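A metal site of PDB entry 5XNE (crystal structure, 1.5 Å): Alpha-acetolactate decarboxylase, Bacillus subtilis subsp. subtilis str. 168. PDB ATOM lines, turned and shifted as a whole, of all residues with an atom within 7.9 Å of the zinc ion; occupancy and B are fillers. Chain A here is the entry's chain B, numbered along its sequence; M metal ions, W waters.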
ATOM      1  N   MET A  10      13.211 -25.242 -28.562  1.00  0.00           N
ATOM      2  CA  MET A  10      13.204 -24.038 -29.370  1.00  0.00           C
ATOM      3  C   MET A  10      12.348 -24.226 -30.609  1.00  0.00           C
ATOM      4  O   MET A  10      11.678 -23.300 -31.055  1.00  0.00           O
ATOM      5  CB  MET A  10      14.636 -23.632 -29.753  1.00  0.00           C
ATOM      6  CG  MET A  10      14.713 -22.352 -30.532  1.00  0.00           C
ATOM      7  SD  MET A  10      14.195 -20.958 -29.516  1.00  0.00           S
ATOM      8  CE  MET A  10      14.204 -19.628 -30.731  1.00  0.00           C
ATOM      9  N   LEU A  13       8.780 -23.375 -29.895  1.00  0.00           N
ATOM     10  CA  LEU A  13       8.623 -21.933 -29.904  1.00  0.00           C
ATOM     11  C   LEU A  13       8.567 -21.405 -31.356  1.00  0.00           C
ATOM     12  O   LEU A  13       7.721 -20.566 -31.682  1.00  0.00           O
ATOM     13  CB  LEU A  13       9.754 -21.282 -29.102  1.00  0.00           C
ATOM     14  CG  LEU A  13       9.473 -19.964 -28.380  1.00  0.00           C
ATOM     15  CD1 LEU A  13       8.424 -20.120 -27.288  1.00  0.00           C
ATOM     16  CD2 LEU A  13      10.789 -19.406 -27.817  1.00  0.00           C
ATOM     17  N   ILE A  35      17.633 -18.460 -18.193  1.00  0.00           N
ATOM     18  CA  ILE A  35      17.063 -17.527 -19.168  1.00  0.00           C
ATOM     19  C   ILE A  35      15.895 -18.190 -19.878  1.00  0.00           C
ATOM     20  O   ILE A  35      15.696 -19.395 -19.785  1.00  0.00           O
ATOM     21  CB  ILE A  35      18.081 -17.061 -20.232  1.00  0.00           C
ATOM     22  CG1 ILE A  35      18.625 -18.250 -21.029  1.00  0.00           C
ATOM     23  CG2 ILE A  35      19.228 -16.273 -19.592  1.00  0.00           C
ATOM     24  CD1 ILE A  35      19.434 -17.829 -22.250  1.00  0.00           C
ATOM     25  N   GLY A  36      15.107 -17.389 -20.589  1.00  0.00           N
ATOM     26  CA  GLY A  36      14.009 -17.952 -21.348  1.00  0.00           C
ATOM     27  C   GLY A  36      12.986 -16.902 -21.652  1.00  0.00           C
ATOM     28  O   GLY A  36      13.286 -15.701 -21.767  1.00  0.00           O
ATOM     29  N   THR A  37      11.747 -17.344 -21.833  1.00  0.00           N
ATOM     30  CA  THR A  37      10.644 -16.416 -22.044  1.00  0.00           C
ATOM     31  C   THR A  37       9.459 -16.869 -21.191  1.00  0.00           C
ATOM     32  O   THR A  37       9.573 -17.750 -20.337  1.00  0.00           O
ATOM     33  CB  THR A  37      10.285 -16.317 -23.537  1.00  0.00           C
ATOM     34  OG1 THR A  37       9.337 -15.269 -23.741  1.00  0.00           O
ATOM     35  CG2 THR A  37       9.740 -17.648 -24.083  1.00  0.00           C
ATOM     36  N   GLU A  44      11.072 -11.262 -21.559  1.00  0.00           N
ATOM     37  CA  GLU A  44      12.288 -12.069 -21.469  1.00  0.00           C
ATOM     38  C   GLU A  44      12.565 -12.465 -20.029  1.00  0.00           C
ATOM     39  O   GLU A  44      12.491 -11.623 -19.118  1.00  0.00           O
ATOM     40  CB  GLU A  44      13.488 -11.288 -22.014  1.00  0.00           C
ATOM     41  CG  GLU A  44      13.271 -10.691 -23.395  1.00  0.00           C
ATOM     42  CD  GLU A  44      13.491 -11.722 -24.499  1.00  0.00           C
ATOM     43  OE1 GLU A  44      14.027 -12.810 -24.195  1.00  0.00           O
ATOM     44  OE2 GLU A  44      13.142 -11.434 -25.659  1.00  0.00           O
ATOM     45  N   LEU A  45      12.905 -13.734 -19.809  1.00  0.00           N
ATOM     46  CA  LEU A  45      13.324 -14.202 -18.487  1.00  0.00           C
ATOM     47  C   LEU A  45      14.845 -14.116 -18.308  1.00  0.00           C
ATOM     48  O   LEU A  45      15.612 -14.512 -19.182  1.00  0.00           O
ATOM     49  CB  LEU A  45      12.881 -15.645 -18.279  1.00  0.00           C
ATOM     50  CG  LEU A  45      13.301 -16.342 -16.992  1.00  0.00           C
ATOM     51  CD1 LEU A  45      12.506 -15.791 -15.839  1.00  0.00           C
ATOM     52  CD2 LEU A  45      13.089 -17.850 -17.083  1.00  0.00           C
ATOM     53  N   PHE A  72       9.250 -22.038 -22.624  1.00  0.00           N
ATOM     54  CA  PHE A  72      10.648 -22.254 -22.999  1.00  0.00           C
ATOM     55  C   PHE A  72      11.561 -21.518 -22.043  1.00  0.00           C
ATOM     56  O   PHE A  72      11.472 -20.300 -21.918  1.00  0.00           O
ATOM     57  CB  PHE A  72      10.917 -21.782 -24.437  1.00  0.00           C
ATOM     58  CG  PHE A  72      12.340 -21.982 -24.877  1.00  0.00           C
ATOM     59  CD1 PHE A  72      12.759 -23.235 -25.286  1.00  0.00           C
ATOM     60  CD2 PHE A  72      13.248 -20.951 -24.857  1.00  0.00           C
ATOM     61  CE1 PHE A  72      14.078 -23.445 -25.691  1.00  0.00           C
ATOM     62  CE2 PHE A  72      14.565 -21.151 -25.260  1.00  0.00           C
ATOM     63  CZ  PHE A  72      14.982 -22.412 -25.680  1.00  0.00           C
ATOM     64  N   ARG A 124      16.799  -7.227 -27.564  1.00  0.00           N
ATOM     65  CA  ARG A 124      15.380  -7.230 -27.886  1.00  0.00           C
ATOM     66  C   ARG A 124      14.584  -7.716 -26.692  1.00  0.00           C
ATOM     67  O   ARG A 124      15.119  -8.416 -25.820  1.00  0.00           O
ATOM     68  CB  ARG A 124      15.056  -8.136 -29.073  1.00  0.00           C
ATOM     69  CG  ARG A 124      15.345  -9.609 -28.785  1.00  0.00           C
ATOM     70  CD  ARG A 124      14.076 -10.449 -28.649  1.00  0.00           C
ATOM     71  NE  ARG A 124      14.430 -11.817 -28.285  1.00  0.00           N
ATOM     72  CZ  ARG A 124      14.547 -12.752 -29.219  1.00  0.00           C
ATOM     73  NH1 ARG A 124      14.315 -12.396 -30.486  1.00  0.00           N
ATOM     74  NH2 ARG A 124      14.902 -14.003 -28.926  1.00  0.00           N
ATOM     75  N   VAL A 126      10.962  -9.795 -26.609  1.00  0.00           N
ATOM     76  CA  VAL A 126       9.721 -10.273 -27.215  1.00  0.00           C
ATOM     77  C   VAL A 126       8.534  -9.739 -26.409  1.00  0.00           C
ATOM     78  O   VAL A 126       8.627  -9.526 -25.193  1.00  0.00           O
ATOM     79  CB  VAL A 126       9.624 -11.813 -27.284  1.00  0.00           C
ATOM     80  CG1 VAL A 126      10.617 -12.367 -28.305  1.00  0.00           C
ATOM     81  CG2 VAL A 126       9.816 -12.435 -25.896  1.00  0.00           C
ATOM     82  N   MET A 136       7.291 -17.858 -34.855  1.00  0.00           N
ATOM     83  CA  MET A 136       8.184 -16.896 -34.210  1.00  0.00           C
ATOM     84  C   MET A 136       8.924 -15.987 -35.194  1.00  0.00           C
ATOM     85  O   MET A 136       9.212 -14.849 -34.861  1.00  0.00           O
ATOM     86  CB  MET A 136       9.199 -17.621 -33.334  1.00  0.00           C
ATOM     87  CG  MET A 136       9.853 -16.677 -32.343  1.00  0.00           C
ATOM     88  SD  MET A 136      10.927 -17.569 -31.220  1.00  0.00           S
ATOM     89  CE  MET A 136      11.630 -16.180 -30.315  1.00  0.00           C
ATOM     90  N   VAL A 169      19.388 -23.319 -28.132  1.00  0.00           N
ATOM     91  CA  VAL A 169      20.029 -22.542 -29.181  1.00  0.00           C
ATOM     92  C   VAL A 169      21.523 -22.817 -29.166  1.00  0.00           C
ATOM     93  O   VAL A 169      22.208 -22.435 -28.218  1.00  0.00           O
ATOM     94  CB  VAL A 169      19.761 -21.029 -28.997  1.00  0.00           C
ATOM     95  CG1 VAL A 169      20.482 -20.244 -30.091  1.00  0.00           C
ATOM     96  CG2 VAL A 169      18.271 -20.741 -29.023  1.00  0.00           C
ATOM     97  N   HIS A 173      23.819 -18.187 -26.033  1.00  0.00           N
ATOM     98  CA  HIS A 173      22.486 -17.613 -25.908  1.00  0.00           C
ATOM     99  C   HIS A 173      22.493 -16.810 -24.608  1.00  0.00           C
ATOM    100  O   HIS A 173      22.591 -17.389 -23.535  1.00  0.00           O
ATOM    101  CB  HIS A 173      21.427 -18.718 -25.905  1.00  0.00           C
ATOM    102  CG  HIS A 173      20.010 -18.220 -25.810  1.00  0.00           C
ATOM    103  ND1 HIS A 173      18.947 -19.059 -25.655  1.00  0.00           N
ATOM    104  CD2 HIS A 173      19.512 -16.961 -25.829  1.00  0.00           C
ATOM    105  CE1 HIS A 173      17.823 -18.353 -25.602  1.00  0.00           C
ATOM    106  NE2 HIS A 173      18.148 -17.071 -25.695  1.00  0.00           N
ATOM    107  N   LEU A 174      22.426 -15.498 -24.731  1.00  0.00           N
ATOM    108  CA  LEU A 174      22.709 -14.593 -23.615  1.00  0.00           C
ATOM    109  C   LEU A 174      21.596 -13.558 -23.451  1.00  0.00           C
ATOM    110  O   LEU A 174      21.087 -13.024 -24.448  1.00  0.00           O
ATOM    111  CB  LEU A 174      24.050 -13.874 -23.823  1.00  0.00           C
ATOM    112  CG  LEU A 174      25.252 -14.771 -24.105  1.00  0.00           C
ATOM    113  CD1 LEU A 174      26.445 -13.900 -24.489  1.00  0.00           C
ATOM    114  CD2 LEU A 174      25.584 -15.618 -22.890  1.00  0.00           C
ATOM    115  N   HIS A 175      21.244 -13.294 -22.195  1.00  0.00           N
ATOM    116  CA  HIS A 175      20.341 -12.197 -21.861  1.00  0.00           C
ATOM    117  C   HIS A 175      21.087 -11.172 -21.008  1.00  0.00           C
ATOM    118  O   HIS A 175      22.164 -11.476 -20.493  1.00  0.00           O
ATOM    119  CB  HIS A 175      19.095 -12.713 -21.134  1.00  0.00           C
ATOM    120  CG  HIS A 175      18.137 -13.460 -22.016  1.00  0.00           C
ATOM    121  ND1 HIS A 175      16.873 -13.811 -21.599  1.00  0.00           N
ATOM    122  CD2 HIS A 175      18.258 -13.914 -23.287  1.00  0.00           C
ATOM    123  CE1 HIS A 175      16.249 -14.446 -22.579  1.00  0.00           C
ATOM    124  NE2 HIS A 175      17.076 -14.535 -23.609  1.00  0.00           N
ATOM    125  N   GLY A 185      17.268  -7.489 -21.817  1.00  0.00           N
ATOM    126  CA  GLY A 185      16.560  -8.366 -22.719  1.00  0.00           C
ATOM    127  C   GLY A 185      17.450  -9.418 -23.328  1.00  0.00           C
ATOM    128  O   GLY A 185      18.485  -9.765 -22.779  1.00  0.00           O
ATOM    129  N   HIS A 186      17.003  -9.971 -24.451  1.00  0.00           N
ATOM    130  CA  HIS A 186      17.756 -10.950 -25.197  1.00  0.00           C
ATOM    131  C   HIS A 186      18.866 -10.236 -25.967  1.00  0.00           C
ATOM    132  O   HIS A 186      18.604  -9.304 -26.702  1.00  0.00           O
ATOM    133  CB  HIS A 186      16.833 -11.716 -26.164  1.00  0.00           C
ATOM    134  CG  HIS A 186      17.563 -12.591 -27.128  1.00  0.00           C
ATOM    135  ND1 HIS A 186      17.703 -13.951 -26.933  1.00  0.00           N
ATOM    136  CD2 HIS A 186      18.168 -12.317 -28.304  1.00  0.00           C
ATOM    137  CE1 HIS A 186      18.372 -14.473 -27.949  1.00  0.00           C
ATOM    138  NE2 HIS A 186      18.676 -13.504 -28.786  1.00  0.00           N
ATOM    139  N   VAL A 187      20.107 -10.695 -25.802  1.00  0.00           N
ATOM    140  CA  VAL A 187      21.262  -9.989 -26.360  1.00  0.00           C
ATOM    141  C   VAL A 187      21.534 -10.333 -27.824  1.00  0.00           C
ATOM    142  O   VAL A 187      21.665 -11.500 -28.170  1.00  0.00           O
ATOM    143  CB  VAL A 187      22.513 -10.319 -25.517  1.00  0.00           C
ATOM    144  CG1 VAL A 187      23.791  -9.734 -26.159  1.00  0.00           C
ATOM    145  CG2 VAL A 187      22.333  -9.787 -24.109  1.00  0.00           C
ATOM    146  N   THR A 232      15.650 -15.704 -35.665  1.00  0.00           N
ATOM    147  CA  THR A 232      14.940 -15.184 -34.510  1.00  0.00           C
ATOM    148  C   THR A 232      15.895 -14.730 -33.406  1.00  0.00           C
ATOM    149  O   THR A 232      15.607 -13.800 -32.651  1.00  0.00           O
ATOM    150  CB  THR A 232      13.943 -16.218 -33.917  1.00  0.00           C
ATOM    151  OG1 THR A 232      14.652 -17.363 -33.433  1.00  0.00           O
ATOM    152  CG2 THR A 232      12.930 -16.669 -34.973  1.00  0.00           C
ATOM    153  N   GLU A 233      17.053 -15.379 -33.321  1.00  0.00           N
ATOM    154  CA  GLU A 233      17.955 -15.119 -32.202  1.00  0.00           C
ATOM    155  C   GLU A 233      19.019 -14.068 -32.490  1.00  0.00           C
ATOM    156  O   GLU A 233      19.672 -13.582 -31.568  1.00  0.00           O
ATOM    157  CB  GLU A 233      18.622 -16.423 -31.768  1.00  0.00           C
ATOM    158  CG  GLU A 233      17.618 -17.508 -31.433  1.00  0.00           C
ATOM    159  CD  GLU A 233      16.646 -17.079 -30.342  1.00  0.00           C
ATOM    160  OE1 GLU A 233      16.990 -17.211 -29.145  1.00  0.00           O
ATOM    161  OE2 GLU A 233      15.531 -16.619 -30.684  1.00  0.00           O
HETATM  162 ZN    ZN M   1      16.571 -15.453 -25.590  1.00  0.00          ZN
HETATM  163  O   HOH W   1      14.600 -14.344 -25.896  1.00  0.00           O
HETATM  164  O   HOH W   2      15.100 -16.829 -24.718  1.00  0.00           O
HETATM  165  O   HOH W   3      15.437 -16.514 -27.248  1.00  0.00           O
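The zinc ion is bound by water W2 (2.2 Å), NE2 of His 175 (2.2 Å), NE2 of His 173 (2.3 Å), water W3 (2.3 Å), water W1 (2.3 Å) and ND1 of His 186 (2.3 Å).
The backbone carbonyl oxygen (O) of Leu 45 is in hydrogen-bond range of a ring nitrogen (ND1) of His 175, 2.8 Å away.
NE2 of His 186 is in hydrogen-bond range of O of Glu 233, 3.0 Å away.
The backbone NH (N) of His 186 sits at hydrogen-bond distance from the backbone carbonyl oxygen (O) of Arg 124 (2.8 Å).
The guanidinium group of Arg 124 is in salt-bridge range of the side-chain carboxylate of Glu 44 (2.9 Å).
OE2 of Glu 44 lies within hydrogen-bond range of N of Val 126, at 2.9 Å.
OE2 of Glu 233 lies within salt-bridge range of NH2 of Arg 124, 3.2 Å away.
The side-chain carboxylate (OE2) of Glu 233 is in hydrogen-bond range of the side-chain hydroxyl (OG1) of Thr 232.
Merely in contact with the zinc ion: Glu 44 (3.9 Å) and Glu 233 (3.99 Å).
Of the 20 residues printed, 5 come within 4 Å of the zinc ion.
Along chain A the residues within 4 Å of the zinc ion span positions 44 to 233.
The nearest printed residue that does not touch the zinc ion is Arg 124 (4.002 Å).
Water W3 lies within hydrogen-bond range of the side-chain carboxylate (OE1) of Glu 233 (2.5 Å) and the guanidinium group (NH2) of Arg 124 (3.1 Å).
Water W1 lies within hydrogen-bond range of NH2 of Arg 124 (3.1 Å) and OE2 of Glu 44 (3.3 Å).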
